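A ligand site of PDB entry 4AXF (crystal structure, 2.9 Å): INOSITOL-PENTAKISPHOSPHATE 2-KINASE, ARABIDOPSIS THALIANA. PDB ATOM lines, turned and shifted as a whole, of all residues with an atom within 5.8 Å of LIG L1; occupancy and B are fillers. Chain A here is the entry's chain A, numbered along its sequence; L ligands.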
ATOM      1  N   ARG A  21      -3.114  26.265  19.381  1.00  0.00           N
ATOM      2  CA  ARG A  21      -4.422  26.894  19.474  1.00  0.00           C
ATOM      3  C   ARG A  21      -4.349  28.100  20.412  1.00  0.00           C
ATOM      4  O   ARG A  21      -4.684  29.226  20.029  1.00  0.00           O
ATOM      5  CB  ARG A  21      -5.464  25.878  19.953  1.00  0.00           C
ATOM      6  CG  ARG A  21      -6.825  26.432  20.332  1.00  0.00           C
ATOM      7  CD  ARG A  21      -7.473  27.233  19.214  1.00  0.00           C
ATOM      8  NE  ARG A  21      -8.834  26.785  18.992  1.00  0.00           N
ATOM      9  CZ  ARG A  21      -9.216  26.022  17.974  1.00  0.00           C
ATOM     10  NH1 ARG A  21      -8.329  25.652  17.056  1.00  0.00           N
ATOM     11  NH2 ARG A  21     -10.471  25.654  17.851  1.00  0.00           N
ATOM     12  N   GLY A  22      -3.894  27.829  21.631  1.00  0.00           N
ATOM     13  CA  GLY A  22      -3.749  28.858  22.653  1.00  0.00           C
ATOM     14  C   GLY A  22      -3.223  28.248  23.945  1.00  0.00           C
ATOM     15  O   GLY A  22      -2.897  27.051  23.996  1.00  0.00           O
ATOM     16  N   GLU A  23      -3.136  29.077  24.981  1.00  0.00           N
ATOM     17  CA  GLU A  23      -2.685  28.659  26.303  1.00  0.00           C
ATOM     18  C   GLU A  23      -3.006  29.703  27.358  1.00  0.00           C
ATOM     19  O   GLU A  23      -3.272  30.855  27.047  1.00  0.00           O
ATOM     20  CB  GLU A  23      -1.181  28.358  26.303  1.00  0.00           C
ATOM     21  CG  GLU A  23      -0.301  29.578  26.088  1.00  0.00           C
ATOM     22  CD  GLU A  23       1.181  29.230  26.077  1.00  0.00           C
ATOM     23  OE1 GLU A  23       1.716  28.794  27.114  1.00  0.00           O
ATOM     24  OE2 GLU A  23       1.803  29.392  25.007  1.00  0.00           O
ATOM     25  N   GLY A  24      -2.982  29.263  28.620  1.00  0.00           N
ATOM     26  CA  GLY A  24      -3.017  30.174  29.746  1.00  0.00           C
ATOM     27  C   GLY A  24      -1.755  29.968  30.562  1.00  0.00           C
ATOM     28  O   GLY A  24      -0.669  29.806  29.993  1.00  0.00           O
ATOM     29  N   GLY A  25      -1.894  29.943  31.879  1.00  0.00           N
ATOM     30  CA  GLY A  25      -0.741  29.768  32.756  1.00  0.00           C
ATOM     31  C   GLY A  25      -0.606  28.359  33.324  1.00  0.00           C
ATOM     32  O   GLY A  25       0.337  28.082  34.058  1.00  0.00           O
ATOM     33  N   ALA A  26      -1.544  27.485  32.975  1.00  0.00           N
ATOM     34  CA  ALA A  26      -1.560  26.130  33.519  1.00  0.00           C
ATOM     35  C   ALA A  26      -1.578  25.058  32.426  1.00  0.00           C
ATOM     36  O   ALA A  26      -0.991  23.986  32.579  1.00  0.00           O
ATOM     37  CB  ALA A  26      -2.741  25.955  34.449  1.00  0.00           C
ATOM     38  N   ASN A  27      -2.272  25.368  31.328  1.00  0.00           N
ATOM     39  CA  ASN A  27      -2.500  24.404  30.263  1.00  0.00           C
ATOM     40  C   ASN A  27      -2.130  24.942  28.883  1.00  0.00           C
ATOM     41  O   ASN A  27      -2.330  26.117  28.592  1.00  0.00           O
ATOM     42  CB  ASN A  27      -3.959  23.955  30.270  1.00  0.00           C
ATOM     43  CG  ASN A  27      -4.337  23.199  31.528  1.00  0.00           C
ATOM     44  OD1 ASN A  27      -4.947  23.758  32.445  1.00  0.00           O
ATOM     45  ND2 ASN A  27      -3.966  21.927  31.594  1.00  0.00           N
ATOM     46  N   LEU A  28      -1.580  24.059  28.054  1.00  0.00           N
ATOM     47  CA  LEU A  28      -1.358  24.339  26.655  1.00  0.00           C
ATOM     48  C   LEU A  28      -2.426  23.602  25.862  1.00  0.00           C
ATOM     49  O   LEU A  28      -2.647  22.403  26.081  1.00  0.00           O
ATOM     50  CB  LEU A  28       0.042  23.899  26.229  1.00  0.00           C
ATOM     51  CG  LEU A  28       0.439  24.032  24.749  1.00  0.00           C
ATOM     52  CD1 LEU A  28       0.629  25.480  24.327  1.00  0.00           C
ATOM     53  CD2 LEU A  28       1.711  23.248  24.467  1.00  0.00           C
ATOM     54  N   VAL A  29      -3.088  24.305  24.941  1.00  0.00           N
ATOM     55  CA  VAL A  29      -4.165  23.716  24.155  1.00  0.00           C
ATOM     56  C   VAL A  29      -3.810  23.611  22.666  1.00  0.00           C
ATOM     57  O   VAL A  29      -3.342  24.578  22.073  1.00  0.00           O
ATOM     58  CB  VAL A  29      -5.505  24.453  24.372  1.00  0.00           C
ATOM     59  CG1 VAL A  29      -6.596  23.884  23.486  1.00  0.00           C
ATOM     60  CG2 VAL A  29      -5.927  24.365  25.833  1.00  0.00           C
ATOM     61  N   VAL A  43      -9.871  19.016  20.781  1.00  0.00           N
ATOM     62  CA  VAL A  43      -8.707  19.768  21.254  1.00  0.00           C
ATOM     63  C   VAL A  43      -8.014  18.995  22.385  1.00  0.00           C
ATOM     64  O   VAL A  43      -8.654  18.204  23.081  1.00  0.00           O
ATOM     65  CB  VAL A  43      -9.069  21.197  21.729  1.00  0.00           C
ATOM     66  CG1 VAL A  43      -9.495  22.071  20.554  1.00  0.00           C
ATOM     67  CG2 VAL A  43     -10.153  21.169  22.803  1.00  0.00           C
ATOM     68  N   ARG A  45      -5.771  19.266  25.895  1.00  0.00           N
ATOM     69  CA  ARG A  45      -5.429  20.148  27.003  1.00  0.00           C
ATOM     70  C   ARG A  45      -4.309  19.512  27.822  1.00  0.00           C
ATOM     71  O   ARG A  45      -4.537  18.590  28.600  1.00  0.00           O
ATOM     72  CB  ARG A  45      -6.659  20.410  27.867  1.00  0.00           C
ATOM     73  CG  ARG A  45      -6.563  21.621  28.776  1.00  0.00           C
ATOM     74  CD  ARG A  45      -7.940  22.038  29.258  1.00  0.00           C
ATOM     75  NE  ARG A  45      -7.892  23.243  30.094  1.00  0.00           N
ATOM     76  CZ  ARG A  45      -7.969  23.255  31.416  1.00  0.00           C
ATOM     77  NH1 ARG A  45      -8.125  22.123  32.106  1.00  0.00           N
ATOM     78  NH2 ARG A  45      -7.914  24.406  32.074  1.00  0.00           N
ATOM     79  N   LYS A  48       1.007  22.191  32.093  1.00  0.00           N
ATOM     80  CA  LYS A  48       2.368  22.707  32.023  1.00  0.00           C
ATOM     81  C   LYS A  48       3.073  22.623  33.379  1.00  0.00           C
ATOM     82  O   LYS A  48       2.435  22.697  34.430  1.00  0.00           O
ATOM     83  CB  LYS A  48       2.359  24.165  31.548  1.00  0.00           C
ATOM     84  CG  LYS A  48       1.799  24.385  30.155  1.00  0.00           C
ATOM     85  CD  LYS A  48       2.174  25.756  29.605  1.00  0.00           C
ATOM     86  CE  LYS A  48       1.358  26.873  30.239  1.00  0.00           C
ATOM     87  NZ  LYS A  48       1.777  28.212  29.742  1.00  0.00           N
ATOM     88  N   ARG A 135       5.811  33.543  27.583  1.00  0.00           N
ATOM     89  CA  ARG A 135       5.159  32.276  27.930  1.00  0.00           C
ATOM     90  C   ARG A 135       6.173  31.138  27.892  1.00  0.00           C
ATOM     91  O   ARG A 135       6.168  30.278  28.779  1.00  0.00           O
ATOM     92  CB  ARG A 135       3.997  31.984  26.971  1.00  0.00           C
ATOM     93  CG  ARG A 135       2.736  32.780  27.257  1.00  0.00           C
ATOM     94  CD  ARG A 135       2.080  32.353  28.562  1.00  0.00           C
ATOM     95  NE  ARG A 135       0.687  32.823  28.642  1.00  0.00           N
ATOM     96  CZ  ARG A 135      -0.038  32.845  29.752  1.00  0.00           C
ATOM     97  NH1 ARG A 135       0.474  32.433  30.907  1.00  0.00           N
ATOM     98  NH2 ARG A 135      -1.286  33.279  29.711  1.00  0.00           N
ATOM     99  N   LEU A 151     -10.951  17.441  24.909  1.00  0.00           N
ATOM    100  CA  LEU A 151     -12.234  18.124  24.935  1.00  0.00           C
ATOM    101  C   LEU A 151     -12.767  18.309  23.525  1.00  0.00           C
ATOM    102  O   LEU A 151     -12.018  18.184  22.551  1.00  0.00           O
ATOM    103  CB  LEU A 151     -12.107  19.483  25.637  1.00  0.00           C
ATOM    104  CG  LEU A 151     -11.217  19.670  26.870  1.00  0.00           C
ATOM    105  CD1 LEU A 151     -11.170  21.145  27.252  1.00  0.00           C
ATOM    106  CD2 LEU A 151     -11.666  18.821  28.046  1.00  0.00           C
ATOM    107  N   ASN A 152     -14.063  18.602  23.412  1.00  0.00           N
ATOM    108  CA  ASN A 152     -14.656  18.982  22.137  1.00  0.00           C
ATOM    109  C   ASN A 152     -14.189  20.367  21.710  1.00  0.00           C
ATOM    110  O   ASN A 152     -14.182  21.304  22.504  1.00  0.00           O
ATOM    111  CB  ASN A 152     -16.185  18.945  22.242  1.00  0.00           C
ATOM    112  CG  ASN A 152     -16.744  17.534  22.128  1.00  0.00           C
ATOM    113  OD1 ASN A 152     -17.344  17.020  23.069  1.00  0.00           O
ATOM    114  ND2 ASN A 152     -16.552  16.899  20.971  1.00  0.00           N
ATOM    115  N   ASP A 153     -13.779  20.483  20.448  1.00  0.00           N
ATOM    116  CA  ASP A 153     -13.358  21.757  19.875  1.00  0.00           C
ATOM    117  C   ASP A 153     -14.573  22.670  19.679  1.00  0.00           C
ATOM    118  O   ASP A 153     -15.309  22.540  18.693  1.00  0.00           O
ATOM    119  CB  ASP A 153     -12.633  21.532  18.550  1.00  0.00           C
ATOM    120  CG  ASP A 153     -12.133  22.826  17.918  1.00  0.00           C
ATOM    121  OD1 ASP A 153     -12.353  23.902  18.506  1.00  0.00           O
ATOM    122  OD2 ASP A 153     -11.526  22.759  16.830  1.00  0.00           O
ATOM    123  N   HIS A 154     -14.759  23.602  20.609  1.00  0.00           N
ATOM    124  CA  HIS A 154     -15.959  24.431  20.643  1.00  0.00           C
ATOM    125  C   HIS A 154     -16.026  25.462  19.544  1.00  0.00           C
ATOM    126  O   HIS A 154     -17.109  26.001  19.255  1.00  0.00           O
ATOM    127  CB  HIS A 154     -16.145  25.062  22.027  1.00  0.00           C
ATOM    128  CG  HIS A 154     -16.332  24.056  23.136  1.00  0.00           C
ATOM    129  ND1 HIS A 154     -17.224  23.048  23.057  1.00  0.00           N
ATOM    130  CD2 HIS A 154     -15.697  23.920  24.375  1.00  0.00           C
ATOM    131  CE1 HIS A 154     -17.161  22.308  24.180  1.00  0.00           C
ATOM    132  NE2 HIS A 154     -16.233  22.849  24.986  1.00  0.00           N
ATOM    133  N   SER A 155     -14.890  25.740  18.894  1.00  0.00           N
ATOM    134  CA  SER A 155     -14.834  26.652  17.751  1.00  0.00           C
ATOM    135  C   SER A 155     -15.516  26.063  16.522  1.00  0.00           C
ATOM    136  O   SER A 155     -15.790  26.780  15.545  1.00  0.00           O
ATOM    137  CB  SER A 155     -13.391  26.992  17.427  1.00  0.00           C
ATOM    138  OG  SER A 155     -12.775  25.907  16.777  1.00  0.00           O
ATOM    139  N   GLU A 171     -14.726  33.712  22.222  1.00  0.00           N
ATOM    140  CA  GLU A 171     -14.251  33.385  23.563  1.00  0.00           C
ATOM    141  C   GLU A 171     -14.239  34.638  24.425  1.00  0.00           C
ATOM    142  O   GLU A 171     -13.729  35.681  24.002  1.00  0.00           O
ATOM    143  CB  GLU A 171     -12.852  32.775  23.506  1.00  0.00           C
ATOM    144  CG  GLU A 171     -12.393  32.155  24.817  1.00  0.00           C
ATOM    145  CD  GLU A 171     -10.899  31.898  24.859  1.00  0.00           C
ATOM    146  OE1 GLU A 171     -10.307  31.657  23.788  1.00  0.00           O
ATOM    147  OE2 GLU A 171     -10.318  31.938  25.967  1.00  0.00           O
ATOM    148  N   LYS A 173     -13.308  35.862  28.474  1.00  0.00           N
ATOM    149  CA  LYS A 173     -12.816  35.671  29.842  1.00  0.00           C
ATOM    150  C   LYS A 173     -13.352  36.835  30.694  1.00  0.00           C
ATOM    151  O   LYS A 173     -12.730  37.893  30.769  1.00  0.00           O
ATOM    152  CB  LYS A 173     -11.283  35.633  29.835  1.00  0.00           C
ATOM    153  CG  LYS A 173     -10.637  35.123  31.118  1.00  0.00           C
ATOM    154  CD  LYS A 173      -9.170  34.817  30.837  1.00  0.00           C
ATOM    155  CE  LYS A 173      -8.269  35.078  32.033  1.00  0.00           C
ATOM    156  NZ  LYS A 173      -8.020  33.873  32.862  1.00  0.00           N
ATOM    157  N   ARG A 246     -11.779  36.872  22.357  1.00  0.00           N
ATOM    158  CA  ARG A 246     -11.253  36.244  21.137  1.00  0.00           C
ATOM    159  C   ARG A 246     -12.388  35.857  20.203  1.00  0.00           C
ATOM    160  O   ARG A 246     -13.518  35.626  20.630  1.00  0.00           O
ATOM    161  CB  ARG A 246     -10.405  35.019  21.471  1.00  0.00           C
ATOM    162  CG  ARG A 246      -9.142  35.339  22.256  1.00  0.00           C
ATOM    163  CD  ARG A 246      -8.254  34.116  22.416  1.00  0.00           C
ATOM    164  NE  ARG A 246      -7.109  34.435  23.263  1.00  0.00           N
ATOM    165  CZ  ARG A 246      -7.044  34.182  24.572  1.00  0.00           C
ATOM    166  NH1 ARG A 246      -8.065  33.597  25.186  1.00  0.00           N
ATOM    167  NH2 ARG A 246      -5.950  34.510  25.255  1.00  0.00           N
ATOM    168  N   PHE A 248     -13.059  33.381  16.521  1.00  0.00           N
ATOM    169  CA  PHE A 248     -12.519  32.366  15.607  1.00  0.00           C
ATOM    170  C   PHE A 248     -13.430  32.147  14.412  1.00  0.00           C
ATOM    171  O   PHE A 248     -14.648  32.025  14.566  1.00  0.00           O
ATOM    172  CB  PHE A 248     -12.357  31.028  16.329  1.00  0.00           C
ATOM    173  CG  PHE A 248     -11.420  31.073  17.500  1.00  0.00           C
ATOM    174  CD1 PHE A 248     -10.062  30.854  17.325  1.00  0.00           C
ATOM    175  CD2 PHE A 248     -11.900  31.301  18.774  1.00  0.00           C
ATOM    176  CE1 PHE A 248      -9.190  30.876  18.401  1.00  0.00           C
ATOM    177  CE2 PHE A 248     -11.035  31.326  19.861  1.00  0.00           C
ATOM    178  CZ  PHE A 248      -9.680  31.114  19.675  1.00  0.00           C
ATOM    179  N   ASP A 373     -11.898  32.848  37.010  1.00  0.00           N
ATOM    180  CA  ASP A 373     -10.845  32.667  36.012  1.00  0.00           C
ATOM    181  C   ASP A 373     -11.204  31.812  34.791  1.00  0.00           C
ATOM    182  O   ASP A 373     -10.370  31.607  33.909  1.00  0.00           O
ATOM    183  CB  ASP A 373      -9.568  32.132  36.673  1.00  0.00           C
ATOM    184  CG  ASP A 373      -8.330  32.438  35.849  1.00  0.00           C
ATOM    185  OD1 ASP A 373      -8.126  33.610  35.480  1.00  0.00           O
ATOM    186  OD2 ASP A 373      -7.549  31.493  35.577  1.00  0.00           O
ATOM    187  N   SER A 375     -13.517  30.738  31.280  1.00  0.00           N
ATOM    188  CA  SER A 375     -13.941  31.433  30.066  1.00  0.00           C
ATOM    189  C   SER A 375     -15.257  30.869  29.525  1.00  0.00           C
ATOM    190  O   SER A 375     -15.762  29.856  30.012  1.00  0.00           O
ATOM    191  CB  SER A 375     -12.854  31.391  29.003  1.00  0.00           C
ATOM    192  OG  SER A 375     -11.773  32.243  29.346  1.00  0.00           O
ATOM    193  N   MET A 377     -17.273  30.176  25.676  1.00  0.00           N
ATOM    194  CA  MET A 377     -17.187  30.125  24.224  1.00  0.00           C
ATOM    195  C   MET A 377     -18.568  30.021  23.592  1.00  0.00           C
ATOM    196  O   MET A 377     -19.266  29.021  23.798  1.00  0.00           O
ATOM    197  CB  MET A 377     -16.300  28.980  23.754  1.00  0.00           C
ATOM    198  CG  MET A 377     -14.822  29.172  24.032  1.00  0.00           C
ATOM    199  SD  MET A 377     -13.791  28.333  22.811  1.00  0.00           S
ATOM    200  CE  MET A 377     -14.067  29.357  21.367  1.00  0.00           C
ATOM    201  N   ILE A 411     -15.298  26.851  29.638  1.00  0.00           N
ATOM    202  CA  ILE A 411     -13.986  26.197  29.563  1.00  0.00           C
ATOM    203  C   ILE A 411     -13.075  26.705  30.675  1.00  0.00           C
ATOM    204  O   ILE A 411     -13.429  27.650  31.382  1.00  0.00           O
ATOM    205  CB  ILE A 411     -13.295  26.416  28.188  1.00  0.00           C
ATOM    206  CG1 ILE A 411     -13.171  27.904  27.877  1.00  0.00           C
ATOM    207  CG2 ILE A 411     -14.036  25.673  27.089  1.00  0.00           C
ATOM    208  CD1 ILE A 411     -12.002  28.277  26.982  1.00  0.00           C
ATOM    209  N   ASP A 412     -11.921  26.070  30.838  1.00  0.00           N
ATOM    210  CA  ASP A 412     -10.888  26.524  31.776  1.00  0.00           C
ATOM    211  C   ASP A 412     -11.395  26.512  33.233  1.00  0.00           C
ATOM    212  O   ASP A 412     -11.313  27.517  33.954  1.00  0.00           O
ATOM    213  CB  ASP A 412     -10.378  27.915  31.358  1.00  0.00           C
ATOM    214  CG  ASP A 412      -9.197  28.399  32.185  1.00  0.00           C
ATOM    215  OD1 ASP A 412      -8.517  27.586  32.846  1.00  0.00           O
ATOM    216  OD2 ASP A 412      -8.959  29.630  32.168  1.00  0.00           O
ATOM    217  N   LEU A 413     -11.927  25.371  33.650  1.00  0.00           N
ATOM    218  CA  LEU A 413     -12.427  25.202  35.005  1.00  0.00           C
ATOM    219  C   LEU A 413     -11.421  24.421  35.856  1.00  0.00           C
ATOM    220  O   LEU A 413     -11.678  23.277  36.261  1.00  0.00           O
ATOM    221  CB  LEU A 413     -13.800  24.520  34.981  1.00  0.00           C
ATOM    222  CG  LEU A 413     -14.956  25.248  34.270  1.00  0.00           C
ATOM    223  CD1 LEU A 413     -16.022  24.269  33.814  1.00  0.00           C
ATOM    224  CD2 LEU A 413     -15.568  26.330  35.146  1.00  0.00           C
ATOM    225  N   SER A 414     -10.268  25.043  36.116  1.00  0.00           N
ATOM    226  CA  SER A 414      -9.162  24.419  36.837  1.00  0.00           C
ATOM    227  C   SER A 414      -9.344  24.472  38.355  1.00  0.00           C
ATOM    228  O   SER A 414     -10.054  25.332  38.875  1.00  0.00           O
ATOM    229  CB  SER A 414      -7.833  25.082  36.468  1.00  0.00           C
ATOM    230  OG  SER A 414      -7.744  25.365  35.079  1.00  0.00           O
ATOM    231  N   LYS A 416      -7.686  25.440  41.759  1.00  0.00           N
ATOM    232  CA  LYS A 416      -6.643  26.315  42.287  1.00  0.00           C
ATOM    233  C   LYS A 416      -6.021  25.692  43.548  1.00  0.00           C
ATOM    234  O   LYS A 416      -6.758  25.268  44.440  1.00  0.00           O
ATOM    235  CB  LYS A 416      -7.193  27.715  42.580  1.00  0.00           C
ATOM    236  CG  LYS A 416      -7.973  28.358  41.427  1.00  0.00           C
ATOM    237  CD  LYS A 416      -7.090  28.610  40.210  1.00  0.00           C
ATOM    238  CE  LYS A 416      -7.916  28.998  38.989  1.00  0.00           C
ATOM    239  NZ  LYS A 416      -7.083  29.247  37.775  1.00  0.00           N
HETATM  240  P1  LIG L   1      -5.649  29.897  32.901  1.00  0.00           P
HETATM  241  O1  LIG L   1      -5.609  28.812  33.969  1.00  0.00           O
HETATM  242  O2  LIG L   1      -6.782  30.891  33.080  1.00  0.00           O
HETATM  243  O3  LIG L   1      -4.325  30.593  32.640  1.00  0.00           O
HETATM  244  P2  LIG L   1      -5.356  27.431  31.085  1.00  0.00           P
HETATM  245  O4  LIG L   1      -3.848  27.530  31.019  1.00  0.00           O
HETATM  246  O5  LIG L   1      -5.943  26.462  32.076  1.00  0.00           O
HETATM  247  N1  LIG L   1      -6.023  29.021  31.410  1.00  0.00           N
HETATM  248  P3  LIG L   1      -7.376  27.164  29.064  1.00  0.00           P
HETATM  249  O6  LIG L   1      -7.855  28.580  29.356  1.00  0.00           O
HETATM  250  O7  LIG L   1      -8.206  25.981  29.525  1.00  0.00           O
HETATM  251  O8  LIG L   1      -5.859  26.972  29.620  1.00  0.00           O
HETATM  252  O9  LIG L   1      -7.170  27.048  27.475  1.00  0.00           O
HETATM  253  C1  LIG L   1      -6.286  27.953  26.811  1.00  0.00           C
HETATM  254  C2  LIG L   1      -6.899  28.425  25.500  1.00  0.00           C
HETATM  255  O10 LIG L   1      -7.157  27.311  24.642  1.00  0.00           O
HETATM  256  C3  LIG L   1      -8.219  29.130  25.712  1.00  0.00           C
HETATM  257  O11 LIG L   1      -8.039  30.543  25.789  1.00  0.00           O
HETATM  258  C4  LIG L   1      -9.050  28.724  24.503  1.00  0.00           C
HETATM  259  O12 LIG L   1      -8.941  29.701  23.455  1.00  0.00           O
HETATM  260  C5  LIG L   1      -8.427  27.435  24.005  1.00  0.00           C
HETATM  261  N2  LIG L   1      -9.327  26.295  24.350  1.00  0.00           N
HETATM  262  C6  LIG L   1      -9.292  25.566  25.487  1.00  0.00           C
HETATM  263  N3  LIG L   1     -10.244  24.602  25.495  1.00  0.00           N
HETATM  264  C7  LIG L   1     -10.922  24.704  24.331  1.00  0.00           C
HETATM  265  C8  LIG L   1     -12.067  23.996  23.688  1.00  0.00           C
HETATM  266  N4  LIG L   1     -12.676  22.960  24.294  1.00  0.00           N
HETATM  267  N5  LIG L   1     -12.464  24.426  22.456  1.00  0.00           N
HETATM  268  C9  LIG L   1     -11.850  25.456  21.828  1.00  0.00           C
HETATM  269  N6  LIG L   1     -10.816  26.141  22.356  1.00  0.00           N
HETATM  270  C10 LIG L   1     -10.318  25.832  23.577  1.00  0.00           C
HETATM  271  C1  LG2 L   2      -3.511  34.590  34.580  1.00  0.00           C
HETATM  272  C2  LG2 L   2      -3.792  33.099  34.715  1.00  0.00           C
HETATM  273  C3  LG2 L   2      -3.827  32.691  36.197  1.00  0.00           C
HETATM  274  P1  LG2 L   2      -3.212  30.119  36.444  1.00  0.00           P
HETATM  275  C4  LG2 L   2      -4.792  33.549  37.017  1.00  0.00           C
HETATM  276  P2  LG2 L   2      -5.859  32.876  39.367  1.00  0.00           P
HETATM  277  C5  LG2 L   2      -4.620  35.054  36.818  1.00  0.00           C
HETATM  278  P3  LG2 L   2      -5.586  36.956  38.442  1.00  0.00           P
HETATM  279  C6  LG2 L   2      -4.565  35.430  35.331  1.00  0.00           C
HETATM  280  P4  LG2 L   2      -5.262  37.827  34.330  1.00  0.00           P
HETATM  281  O1  LG2 L   2      -3.452  34.955  33.193  1.00  0.00           O
HETATM  282  O2  LG2 L   2      -5.045  32.757  34.097  1.00  0.00           O
HETATM  283  O3  LG2 L   2      -4.258  31.339  36.312  1.00  0.00           O
HETATM  284  O4  LG2 L   2      -4.618  33.187  38.389  1.00  0.00           O
HETATM  285  O5  LG2 L   2      -5.733  35.726  37.411  1.00  0.00           O
HETATM  286  O6  LG2 L   2      -4.308  36.821  35.181  1.00  0.00           O
HETATM  287  O7  LG2 L   2      -2.987  29.717  35.008  1.00  0.00           O
HETATM  288  O8  LG2 L   2      -5.509  31.575  40.063  1.00  0.00           O
HETATM  289  O9  LG2 L   2      -4.936  38.071  37.669  1.00  0.00           O
HETATM  290  O10 LG2 L   2      -4.450  38.092  33.072  1.00  0.00           O
HETATM  291  O11 LG2 L   2      -1.993  30.722  37.136  1.00  0.00           O
HETATM  292  O12 LG2 L   2      -7.044  32.750  38.445  1.00  0.00           O
HETATM  293  O13 LG2 L   2      -7.031  37.249  38.808  1.00  0.00           O
HETATM  294  O14 LG2 L   2      -6.563  37.096  34.098  1.00  0.00           O
HETATM  295  O15 LG2 L   2      -3.955  29.073  37.259  1.00  0.00           O
HETATM  296  O16 LG2 L   2      -5.918  34.074  40.275  1.00  0.00           O
HETATM  297  O17 LG2 L   2      -4.713  36.434  39.554  1.00  0.00           O
HETATM  298  O18 LG2 L   2      -5.396  39.025  35.224  1.00  0.00           O
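The side-chain sulfur of Met 377 lies close to a nitrogen (N6) of LIG L1.
Merely in contact with LIG L1: Arg 21 (3.96 Å), Gly 22 (3.995 Å), Glu 23 (3.7 Å), Val 29 (3.3 Å), Val 43 (3.4 Å), Leu 151 (3.8 Å), Asp 153 (3.7 Å), Ile 411 (3.9 Å) and Ser 414 (3.7 Å).
Hydrophobic or aromatic side chains within 4 Å of LIG L1: Ala 26, Val 29, Val 43, Leu 151, His 154, Met 377 and Ile 411.
The side-chain carboxylate of Glu 171 sits at hydrogen-bond distance from an oxygen (O12) of LIG L1, at 2.4 Å.
O3 of LIG L1 lies within hydrogen-bond range of N of Gly 25 (2.6 Å).
A nitrogen (N1) of LIG L1 sits at hydrogen-bond distance from the side-chain carboxylate (OD2) of Asp 412.
An oxygen (O2) of LIG L1 lies close to the side-chain carboxylate of Asp 373 (2.7 Å).
The backbone NH (N) of Asn 27 sits at hydrogen-bond distance from an oxygen (O4) of LIG L1, 2.7 Å away.
The side-chain amide oxygen of Asn 27 lies close to an oxygen (O5) of LIG L1, 2.9 Å away.
The guanidinium group (NE) of Arg 45 lies within salt-bridge range of an oxygen (O7) of LIG L1 (2.8 Å).
N4 of LIG L1 is in hydrogen-bond range of O of Asn 152, at 2.9 Å.
An oxygen (O4) of LIG L1 is in hydrogen-bond range of the backbone NH (N) of Ala 26, at 3.0 Å.
The backbone NH (N) of Gly 24 lies close to an oxygen (O4) of LIG L1.
N5 of LIG L1 sits at hydrogen-bond distance from N of His 154, 3.1 Å away.
NH1 of Arg 246 lies within hydrogen-bond range of O11 of LIG L1.
An oxygen (O2) of LIG L1 is in salt-bridge range of the side-chain amino group of Lys 173.
An oxygen (O7) of LG2 L2 lies close to the backbone NH (N) of Gly 25 (3.3 Å).
The side-chain carboxylate of Asp 373 lies within hydrogen-bond range of an oxygen (O2) of LG2 L2, 3.2 Å away.
The backbone NH (N) of Ala 26 sits at hydrogen-bond distance from an oxygen (O7) of LG2 L2 (3.3 Å).
An oxygen (O14) of LG2 L2 is in salt-bridge range of the side-chain amino group (NZ) of Lys 173 (3.7 Å).
O15 of LG2 L2 is in salt-bridge range of NZ of Lys 416 (3.2 Å).
NH1 of Arg 246 is in salt-bridge range of OE2 of Glu 171.
OD1 of Asp 412 lies within salt-bridge range of NH2 of Arg 45, at 3.3 Å.
The side-chain hydroxyl (OG) of Ser 414 lies within hydrogen-bond range of the side-chain carboxylate (OD1) of Asp 412 (3.2 Å).
NH1 of Arg 135 lies within hydrogen-bond range of O of Gly 24, 3.0 Å away.
The guanidinium group (NH2) of Arg 21 lies within salt-bridge range of the side-chain carboxylate (OD1) of Asp 153 (2.7 Å).
The side-chain hydroxyl (OG) of Ser 155 is in hydrogen-bond range of the side-chain carboxylate (OD1) of Asp 153.
The side-chain carboxylate (OE1) of Glu 23 is in salt-bridge range of the side-chain amino group (NZ) of Lys 48 (2.7 Å).
N of Ile 411 lies within hydrogen-bond range of O of Ser 375, at 3.1 Å.
An oxygen (O3) of LIG L1 lies within hydrogen-bond range of an oxygen (O2) of LG2 L2 (2.7 Å).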
